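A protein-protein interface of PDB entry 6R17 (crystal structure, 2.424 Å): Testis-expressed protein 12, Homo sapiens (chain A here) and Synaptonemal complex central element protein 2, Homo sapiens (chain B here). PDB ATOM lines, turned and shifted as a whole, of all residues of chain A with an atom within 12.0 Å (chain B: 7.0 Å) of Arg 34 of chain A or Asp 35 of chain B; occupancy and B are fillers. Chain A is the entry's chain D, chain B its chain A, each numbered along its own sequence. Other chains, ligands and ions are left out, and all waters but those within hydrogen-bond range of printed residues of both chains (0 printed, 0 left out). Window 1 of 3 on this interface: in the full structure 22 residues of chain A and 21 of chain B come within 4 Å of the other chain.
Hydrophobic or aromatic side chains of chain A within 4 Å of the printed part of chain B: Tyr 27, Leu 31, Val 37 and Tyr 41. Along chain A the printed residues that touch a printed residue of chain B span positions 27 to 41. Hydrophobic or aromatic side chains of chain B that line the printed part of chain A: Leu 38 and Met 39. Among the printed residues, Asp or Glu carboxylates within 4 Å of a Lys or Arg side-chain nitrogen of the other chain: Arg 34 of chain A with Asp 35 of chain B and Asp 38 of chain A with Arg 32 of chain B.
The guanidinium group of Arg 32 of chain B lies within salt-bridge range of the side-chain carboxylate of Asp 38 of chain A (2.6 Å). OD2 of Asp 35 of chain B is in salt-bridge range of NH2 of Arg 34 of chain A (2.6 Å).
Among the printed residues, merely in contact across the chains: Tyr 27 of chain A with Met 39 of chain B (3.7 Å), Leu 31 of chain A with Met 39 of chain B (3.8 Å), Arg 34 of chain A with Ser 31 of chain B (3.9 Å), Arg 34 of chain A with Lys 34 of chain B (3.5 Å), Arg 34 of chain A with Leu 38 of chain B (3.8 Å), Val 37 of chain A with Ser 31 of chain B (3.8 Å) and Tyr 41 of chain A with Ser 31 of chain B (3.7 Å).
Of chain B, only Ser 31 (3.9 Å), Lys 34 (3.5 Å), Asp 35 (2.6 Å) and Leu 38 (3.8 Å) come within 4 Å of Arg 34 of chain A. Asp 35 of chain B touches just one residue of chain A: Arg 34 (2.6 Å). Of chain A, only Arg 34, Val 37 and Tyr 41 come within 4 Å of Ser 31 of chain B. Arg 32 of chain B touches just one residue of chain A: Asp 38 (2.6 Å). No residue of chain A comes within 4 Å of His 36 of chain B. No residue of chain A comes within 4 Å of Ala 37 of chain B. Of chain A, only Arg 34 comes within 4 Å of Leu 38 of chain B. Of the printed residues of chain B, Val 37 of chain A touches Ser 31. Printed residues of chain B within 4 Å of Asp 38 of chain A: Arg 32 (2.6 Å). Printed residues of chain B within 4 Å of Leu 31 of chain A: Met 39 (3.8 Å).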
ATOM      1  N   SER A  25      37.830  23.257  15.504  1.00  0.00           N
ATOM      2  CA  SER A  25      36.994  22.079  15.250  1.00  0.00           C
ATOM      3  C   SER A  25      36.642  21.350  16.552  1.00  0.00           C
ATOM      4  O   SER A  25      35.529  20.822  16.692  1.00  0.00           O
ATOM      5  CB  SER A  25      37.665  21.142  14.236  1.00  0.00           C
ATOM      6  OG  SER A  25      37.864  21.783  12.978  1.00  0.00           O
ATOM      7  N   THR A  26      37.575  21.289  17.513  1.00  0.00           N
ATOM      8  CA  THR A  26      37.250  20.712  18.820  1.00  0.00           C
ATOM      9  C   THR A  26      36.163  21.528  19.520  1.00  0.00           C
ATOM     10  O   THR A  26      35.255  20.968  20.159  1.00  0.00           O
ATOM     11  CB  THR A  26      38.514  20.615  19.685  1.00  0.00           C
ATOM     12  OG1 THR A  26      39.386  19.616  19.141  1.00  0.00           O
ATOM     13  CG2 THR A  26      38.168  20.241  21.107  1.00  0.00           C
ATOM     14  N   TYR A  27      36.215  22.855  19.373  1.00  0.00           N
ATOM     15  CA  TYR A  27      35.152  23.697  19.910  1.00  0.00           C
ATOM     16  C   TYR A  27      33.819  23.369  19.250  1.00  0.00           C
ATOM     17  O   TYR A  27      32.814  23.155  19.939  1.00  0.00           O
ATOM     18  CB  TYR A  27      35.508  25.171  19.698  1.00  0.00           C
ATOM     19  CG  TYR A  27      34.608  26.147  20.415  1.00  0.00           C
ATOM     20  CD1 TYR A  27      34.104  25.865  21.676  1.00  0.00           C
ATOM     21  CD2 TYR A  27      34.254  27.350  19.821  1.00  0.00           C
ATOM     22  CE1 TYR A  27      33.280  26.757  22.329  1.00  0.00           C
ATOM     23  CE2 TYR A  27      33.431  28.246  20.464  1.00  0.00           C
ATOM     24  CZ  TYR A  27      32.946  27.946  21.717  1.00  0.00           C
ATOM     25  OH  TYR A  27      32.126  28.849  22.349  1.00  0.00           O
ATOM     26  N   ALA A  28      33.819  23.229  17.921  1.00  0.00           N
ATOM     27  CA  ALA A  28      32.596  22.875  17.205  1.00  0.00           C
ATOM     28  C   ALA A  28      32.026  21.549  17.696  1.00  0.00           C
ATOM     29  O   ALA A  28      30.804  21.405  17.854  1.00  0.00           O
ATOM     30  CB  ALA A  28      32.875  22.811  15.705  1.00  0.00           C
ATOM     31  N   LYS A  29      32.895  20.565  17.935  1.00  0.00           N
ATOM     32  CA  LYS A  29      32.423  19.263  18.403  1.00  0.00           C
ATOM     33  C   LYS A  29      31.767  19.381  19.772  1.00  0.00           C
ATOM     34  O   LYS A  29      30.684  18.826  20.000  1.00  0.00           O
ATOM     35  CB  LYS A  29      33.587  18.275  18.451  1.00  0.00           C
ATOM     36  CG  LYS A  29      33.270  16.918  19.064  1.00  0.00           C
ATOM     37  CD  LYS A  29      34.394  15.933  18.761  1.00  0.00           C
ATOM     38  CE  LYS A  29      35.726  16.391  19.351  1.00  0.00           C
ATOM     39  NZ  LYS A  29      36.857  15.499  18.954  1.00  0.00           N
ATOM     40  N   LEU A  30      32.438  20.063  20.704  1.00  0.00           N
ATOM     41  CA  LEU A  30      31.852  20.380  22.006  1.00  0.00           C
ATOM     42  C   LEU A  30      30.448  20.955  21.868  1.00  0.00           C
ATOM     43  O   LEU A  30      29.498  20.521  22.547  1.00  0.00           O
ATOM     44  CB  LEU A  30      32.747  21.414  22.678  1.00  0.00           C
ATOM     45  CG  LEU A  30      32.395  22.088  23.991  1.00  0.00           C
ATOM     46  CD1 LEU A  30      32.296  21.070  25.095  1.00  0.00           C
ATOM     47  CD2 LEU A  30      33.388  23.229  24.298  1.00  0.00           C
ATOM     48  N   LEU A  31      30.303  21.913  20.957  1.00  0.00           N
ATOM     49  CA  LEU A  31      29.033  22.604  20.769  1.00  0.00           C
ATOM     50  C   LEU A  31      27.955  21.629  20.310  1.00  0.00           C
ATOM     51  O   LEU A  31      26.832  21.609  20.845  1.00  0.00           O
ATOM     52  CB  LEU A  31      29.270  23.715  19.750  1.00  0.00           C
ATOM     53  CG  LEU A  31      30.417  24.625  20.237  1.00  0.00           C
ATOM     54  CD1 LEU A  31      30.960  25.586  19.156  1.00  0.00           C
ATOM     55  CD2 LEU A  31      30.049  25.376  21.522  1.00  0.00           C
ATOM     56  N   SER A  32      28.306  20.773  19.345  1.00  0.00           N
ATOM     57  CA  SER A  32      27.369  19.762  18.864  1.00  0.00           C
ATOM     58  C   SER A  32      26.958  18.801  19.976  1.00  0.00           C
ATOM     59  O   SER A  32      25.776  18.459  20.098  1.00  0.00           O
ATOM     60  CB  SER A  32      27.975  18.997  17.687  1.00  0.00           C
ATOM     61  OG  SER A  32      28.098  19.839  16.559  1.00  0.00           O
ATOM     62  N   GLU A  33      27.916  18.347  20.791  1.00  0.00           N
ATOM     63  CA  GLU A  33      27.578  17.393  21.851  1.00  0.00           C
ATOM     64  C   GLU A  33      26.580  18.000  22.834  1.00  0.00           C
ATOM     65  O   GLU A  33      25.601  17.347  23.242  1.00  0.00           O
ATOM     66  CB  GLU A  33      28.840  16.930  22.595  1.00  0.00           C
ATOM     67  CG  GLU A  33      30.052  16.526  21.736  1.00  0.00           C
ATOM     68  CD  GLU A  33      29.916  15.182  21.029  1.00  0.00           C
ATOM     69  OE1 GLU A  33      28.809  14.846  20.559  1.00  0.00           O
ATOM     70  OE2 GLU A  33      30.932  14.458  20.931  1.00  0.00           O
ATOM     71  N   ARG A  34      26.795  19.262  23.211  1.00  0.00           N
ATOM     72  CA  ARG A  34      25.880  19.883  24.164  1.00  0.00           C
ATOM     73  C   ARG A  34      24.484  20.049  23.556  1.00  0.00           C
ATOM     74  O   ARG A  34      23.462  19.759  24.212  1.00  0.00           O
ATOM     75  CB  ARG A  34      26.456  21.219  24.641  1.00  0.00           C
ATOM     76  CG  ARG A  34      27.847  21.086  25.262  1.00  0.00           C
ATOM     77  CD  ARG A  34      27.891  20.059  26.396  1.00  0.00           C
ATOM     78  NE  ARG A  34      26.814  20.207  27.371  1.00  0.00           N
ATOM     79  CZ  ARG A  34      26.538  19.311  28.316  1.00  0.00           C
ATOM     80  NH1 ARG A  34      27.265  18.206  28.417  1.00  0.00           N
ATOM     81  NH2 ARG A  34      25.540  19.522  29.164  1.00  0.00           N
ATOM     82  N   ALA A  35      24.420  20.469  22.287  1.00  0.00           N
ATOM     83  CA  ALA A  35      23.122  20.550  21.620  1.00  0.00           C
ATOM     84  C   ALA A  35      22.432  19.189  21.563  1.00  0.00           C
ATOM     85  O   ALA A  35      21.199  19.103  21.686  1.00  0.00           O
ATOM     86  CB  ALA A  35      23.294  21.122  20.212  1.00  0.00           C
ATOM     87  N   ALA A  36      23.208  18.113  21.401  1.00  0.00           N
ATOM     88  CA  ALA A  36      22.627  16.773  21.398  1.00  0.00           C
ATOM     89  C   ALA A  36      21.983  16.453  22.740  1.00  0.00           C
ATOM     90  O   ALA A  36      20.912  15.833  22.796  1.00  0.00           O
ATOM     91  CB  ALA A  36      23.694  15.734  21.051  1.00  0.00           C
ATOM     92  N   VAL A  37      22.628  16.857  23.837  1.00  0.00           N
ATOM     93  CA  VAL A  37      22.022  16.646  25.155  1.00  0.00           C
ATOM     94  C   VAL A  37      20.666  17.350  25.235  1.00  0.00           C
ATOM     95  O   VAL A  37      19.669  16.793  25.741  1.00  0.00           O
ATOM     96  CB  VAL A  37      22.975  17.126  26.265  1.00  0.00           C
ATOM     97  CG1 VAL A  37      22.306  17.006  27.628  1.00  0.00           C
ATOM     98  CG2 VAL A  37      24.277  16.342  26.226  1.00  0.00           C
ATOM     99  N   ASP A  38      20.607  18.584  24.730  1.00  0.00           N
ATOM    100  CA  ASP A  38      19.336  19.313  24.737  1.00  0.00           C
ATOM    101  C   ASP A  38      18.256  18.559  23.951  1.00  0.00           C
ATOM    102  O   ASP A  38      17.099  18.434  24.397  1.00  0.00           O
ATOM    103  CB  ASP A  38      19.553  20.717  24.167  1.00  0.00           C
ATOM    104  CG  ASP A  38      18.604  21.748  24.750  1.00  0.00           C
ATOM    105  OD1 ASP A  38      18.652  21.988  25.975  1.00  0.00           O
ATOM    106  OD2 ASP A  38      17.821  22.334  23.973  1.00  0.00           O
ATOM    107  N   ALA A  39      18.626  18.015  22.790  1.00  0.00           N
ATOM    108  CA  ALA A  39      17.658  17.248  22.003  1.00  0.00           C
ATOM    109  C   ALA A  39      17.183  16.003  22.758  1.00  0.00           C
ATOM    110  O   ALA A  39      16.023  15.577  22.625  1.00  0.00           O
ATOM    111  CB  ALA A  39      18.265  16.870  20.652  1.00  0.00           C
ATOM    112  N   SER A  40      18.074  15.391  23.538  1.00  0.00           N
ATOM    113  CA  SER A  40      17.662  14.247  24.352  1.00  0.00           C
ATOM    114  C   SER A  40      16.565  14.638  25.341  1.00  0.00           C
ATOM    115  O   SER A  40      15.597  13.887  25.552  1.00  0.00           O
ATOM    116  CB  SER A  40      18.872  13.663  25.076  1.00  0.00           C
ATOM    117  OG  SER A  40      18.483  12.679  26.013  1.00  0.00           O
ATOM    118  N   TYR A  41      16.692  15.821  25.949  1.00  0.00           N
ATOM    119  CA  TYR A  41      15.599  16.310  26.794  1.00  0.00           C
ATOM    120  C   TYR A  41      14.303  16.500  25.997  1.00  0.00           C
ATOM    121  O   TYR A  41      13.194  16.268  26.521  1.00  0.00           O
ATOM    122  CB  TYR A  41      16.021  17.582  27.528  1.00  0.00           C
ATOM    123  CG  TYR A  41      16.867  17.280  28.746  1.00  0.00           C
ATOM    124  CD1 TYR A  41      16.783  16.038  29.364  1.00  0.00           C
ATOM    125  CD2 TYR A  41      17.699  18.238  29.313  1.00  0.00           C
ATOM    126  CE1 TYR A  41      17.531  15.744  30.488  1.00  0.00           C
ATOM    127  CE2 TYR A  41      18.452  17.952  30.443  1.00  0.00           C
ATOM    128  CZ  TYR A  41      18.364  16.706  31.025  1.00  0.00           C
ATOM    129  OH  TYR A  41      19.114  16.428  32.148  1.00  0.00           O
ATOM    130  N   ILE A  42      14.417  16.918  24.731  1.00  0.00           N
ATOM    131  CA  ILE A  42      13.209  16.992  23.898  1.00  0.00           C
ATOM    132  C   ILE A  42      12.529  15.620  23.828  1.00  0.00           C
ATOM    133  O   ILE A  42      11.299  15.490  23.988  1.00  0.00           O
ATOM    134  CB  ILE A  42      13.550  17.513  22.485  1.00  0.00           C
ATOM    135  CG1 ILE A  42      13.882  19.000  22.529  1.00  0.00           C
ATOM    136  CG2 ILE A  42      12.405  17.241  21.515  1.00  0.00           C
ATOM    137  CD1 ILE A  42      14.215  19.595  21.180  1.00  0.00           C
ATOM    138  N   ASP A  43      13.320  14.569  23.605  1.00  0.00           N
ATOM    139  CA  ASP A  43      12.733  13.227  23.539  1.00  0.00           C
ATOM    140  C   ASP A  43      12.117  12.800  24.874  1.00  0.00           C
ATOM    141  O   ASP A  43      11.130  12.045  24.899  1.00  0.00           O
ATOM    142  CB  ASP A  43      13.776  12.206  23.083  1.00  0.00           C
ATOM    143  CG  ASP A  43      13.913  12.153  21.576  1.00  0.00           C
ATOM    144  OD1 ASP A  43      13.101  12.801  20.880  1.00  0.00           O
ATOM    145  OD2 ASP A  43      14.829  11.463  21.087  1.00  0.00           O
ATOM    146  N   ASN B  29      16.894  23.680  32.540  1.00  0.00           N
ATOM    147  CA  ASN B  29      17.527  24.929  32.962  1.00  0.00           C
ATOM    148  C   ASN B  29      18.958  24.689  33.436  1.00  0.00           C
ATOM    149  O   ASN B  29      19.892  25.403  33.036  1.00  0.00           O
ATOM    150  CB  ASN B  29      16.704  25.594  34.066  1.00  0.00           C
ATOM    151  CG  ASN B  29      15.416  26.200  33.549  1.00  0.00           C
ATOM    152  OD1 ASN B  29      15.385  26.803  32.476  1.00  0.00           O
ATOM    153  ND2 ASN B  29      14.344  26.050  34.319  1.00  0.00           N
ATOM    154  N   LYS B  30      19.147  23.699  34.315  1.00  0.00           N
ATOM    155  CA  LYS B  30      20.501  23.403  34.781  1.00  0.00           C
ATOM    156  C   LYS B  30      21.403  22.978  33.628  1.00  0.00           C
ATOM    157  O   LYS B  30      22.589  23.329  33.599  1.00  0.00           O
ATOM    158  CB  LYS B  30      20.493  22.339  35.882  1.00  0.00           C
ATOM    159  CG  LYS B  30      19.754  22.752  37.145  1.00  0.00           C
ATOM    160  CD  LYS B  30      20.169  21.897  38.339  1.00  0.00           C
ATOM    161  CE  LYS B  30      19.173  20.795  38.644  1.00  0.00           C
ATOM    162  NZ  LYS B  30      19.491  19.557  37.883  1.00  0.00           N
ATOM    163  N   SER B  31      20.868  22.205  32.679  1.00  0.00           N
ATOM    164  CA  SER B  31      21.658  21.799  31.521  1.00  0.00           C
ATOM    165  C   SER B  31      22.076  23.005  30.687  1.00  0.00           C
ATOM    166  O   SER B  31      23.202  23.055  30.179  1.00  0.00           O
ATOM    167  CB  SER B  31      20.867  20.804  30.671  1.00  0.00           C
ATOM    168  OG  SER B  31      21.706  20.166  29.724  1.00  0.00           O
ATOM    169  N   ARG B  32      21.183  23.987  30.536  1.00  0.00           N
ATOM    170  CA  ARG B  32      21.541  25.203  29.810  1.00  0.00           C
ATOM    171  C   ARG B  32      22.660  25.950  30.521  1.00  0.00           C
ATOM    172  O   ARG B  32      23.600  26.440  29.882  1.00  0.00           O
ATOM    173  CB  ARG B  32      20.322  26.116  29.663  1.00  0.00           C
ATOM    174  CG  ARG B  32      19.204  25.606  28.773  1.00  0.00           C
ATOM    175  CD  ARG B  32      19.650  25.451  27.331  1.00  0.00           C
ATOM    176  NE  ARG B  32      18.683  24.682  26.556  1.00  0.00           N
ATOM    177  CZ  ARG B  32      17.682  25.228  25.872  1.00  0.00           C
ATOM    178  NH1 ARG B  32      17.519  26.544  25.876  1.00  0.00           N
ATOM    179  NH2 ARG B  32      16.841  24.463  25.192  1.00  0.00           N
ATOM    180  N   GLN B  33      22.571  26.045  31.850  1.00  0.00           N
ATOM    181  CA  GLN B  33      23.622  26.716  32.615  1.00  0.00           C
ATOM    182  C   GLN B  33      24.961  26.001  32.461  1.00  0.00           C
ATOM    183  O   GLN B  33      26.005  26.640  32.254  1.00  0.00           O
ATOM    184  CB  GLN B  33      23.216  26.788  34.086  1.00  0.00           C
ATOM    185  CG  GLN B  33      22.211  27.882  34.388  1.00  0.00           C
ATOM    186  CD  GLN B  33      21.708  27.828  35.815  1.00  0.00           C
ATOM    187  OE1 GLN B  33      22.305  27.182  36.675  1.00  0.00           O
ATOM    188  NE2 GLN B  33      20.597  28.506  36.072  1.00  0.00           N
ATOM    189  N   LYS B  34      24.944  24.669  32.553  1.00  0.00           N
ATOM    190  CA  LYS B  34      26.163  23.884  32.389  1.00  0.00           C
ATOM    191  C   LYS B  34      26.757  24.093  30.999  1.00  0.00           C
ATOM    192  O   LYS B  34      27.977  24.267  30.853  1.00  0.00           O
ATOM    193  CB  LYS B  34      25.862  22.410  32.671  1.00  0.00           C
ATOM    194  CG  LYS B  34      27.027  21.453  32.507  1.00  0.00           C
ATOM    195  CD  LYS B  34      26.533  20.006  32.466  1.00  0.00           C
ATOM    196  CE  LYS B  34      27.688  19.020  32.419  1.00  0.00           C
ATOM    197  NZ  LYS B  34      27.214  17.606  32.373  1.00  0.00           N
ATOM    198  N   ASP B  35      25.904  24.098  29.966  1.00  0.00           N
ATOM    199  CA  ASP B  35      26.391  24.300  28.605  1.00  0.00           C
ATOM    200  C   ASP B  35      27.016  25.679  28.450  1.00  0.00           C
ATOM    201  O   ASP B  35      28.050  25.828  27.791  1.00  0.00           O
ATOM    202  CB  ASP B  35      25.257  24.140  27.586  1.00  0.00           C
ATOM    203  CG  ASP B  35      24.727  22.726  27.505  1.00  0.00           C
ATOM    204  OD1 ASP B  35      23.952  22.438  26.565  1.00  0.00           O
ATOM    205  OD2 ASP B  35      25.051  21.914  28.392  1.00  0.00           O
ATOM    206  N   HIS B  36      26.396  26.701  29.048  1.00  0.00           N
ATOM    207  CA  HIS B  36      26.931  28.057  28.950  1.00  0.00           C
ATOM    208  C   HIS B  36      28.294  28.162  29.622  1.00  0.00           C
ATOM    209  O   HIS B  36      29.224  28.777  29.080  1.00  0.00           O
ATOM    210  CB  HIS B  36      25.950  29.053  29.570  1.00  0.00           C
ATOM    211  CG  HIS B  36      26.528  30.418  29.782  1.00  0.00           C
ATOM    212  ND1 HIS B  36      26.694  31.324  28.757  1.00  0.00           N
ATOM    213  CD2 HIS B  36      26.977  31.031  30.902  1.00  0.00           C
ATOM    214  CE1 HIS B  36      27.220  32.437  29.236  1.00  0.00           C
ATOM    215  NE2 HIS B  36      27.402  32.285  30.535  1.00  0.00           N
ATOM    216  N   ALA B  37      28.433  27.574  30.813  1.00  0.00           N
ATOM    217  CA  ALA B  37      29.728  27.616  31.488  1.00  0.00           C
ATOM    218  C   ALA B  37      30.801  26.916  30.662  1.00  0.00           C
ATOM    219  O   ALA B  37      31.922  27.432  30.507  1.00  0.00           O
ATOM    220  CB  ALA B  37      29.623  26.981  32.873  1.00  0.00           C
ATOM    221  N   LEU B  38      30.472  25.743  30.108  1.00  0.00           N
ATOM    222  CA  LEU B  38      31.438  25.009  29.299  1.00  0.00           C
ATOM    223  C   LEU B  38      31.853  25.826  28.072  1.00  0.00           C
ATOM    224  O   LEU B  38      33.036  25.920  27.749  1.00  0.00           O
ATOM    225  CB  LEU B  38      30.853  23.664  28.870  1.00  0.00           C
ATOM    226  CG  LEU B  38      30.524  22.627  29.948  1.00  0.00           C
ATOM    227  CD1 LEU B  38      30.097  21.326  29.285  1.00  0.00           C
ATOM    228  CD2 LEU B  38      31.707  22.408  30.871  1.00  0.00           C
ATOM    229  N   MET B  39      30.861  26.410  27.391  1.00  0.00           N
ATOM    230  CA  MET B  39      31.154  27.257  26.235  1.00  0.00           C
ATOM    231  C   MET B  39      32.105  28.398  26.596  1.00  0.00           C
ATOM    232  O   MET B  39      33.117  28.607  25.914  1.00  0.00           O
ATOM    233  CB  MET B  39      29.847  27.804  25.641  1.00  0.00           C
ATOM    234  CG  MET B  39      28.984  26.779  24.911  1.00  0.00           C
ATOM    235  SD  MET B  39      27.297  27.366  24.617  1.00  0.00           S
ATOM    236  CE  MET B  39      26.464  25.827  24.227  1.00  0.00           C
ATOM    237  N   THR B  40      31.813  29.136  27.672  1.00  0.00           N
ATOM    238  CA  THR B  40      32.619  30.314  28.001  1.00  0.00           C
ATOM    239  C   THR B  40      34.046  29.935  28.388  1.00  0.00           C
ATOM    240  O   THR B  40      35.007  30.612  27.988  1.00  0.00           O
ATOM    241  CB  THR B  40      31.962  31.089  29.140  1.00  0.00           C
ATOM    242  OG1 THR B  40      31.781  30.173  30.220  1.00  0.00           O
ATOM    243  CG2 THR B  40      30.598  31.604  28.698  1.00  0.00           C
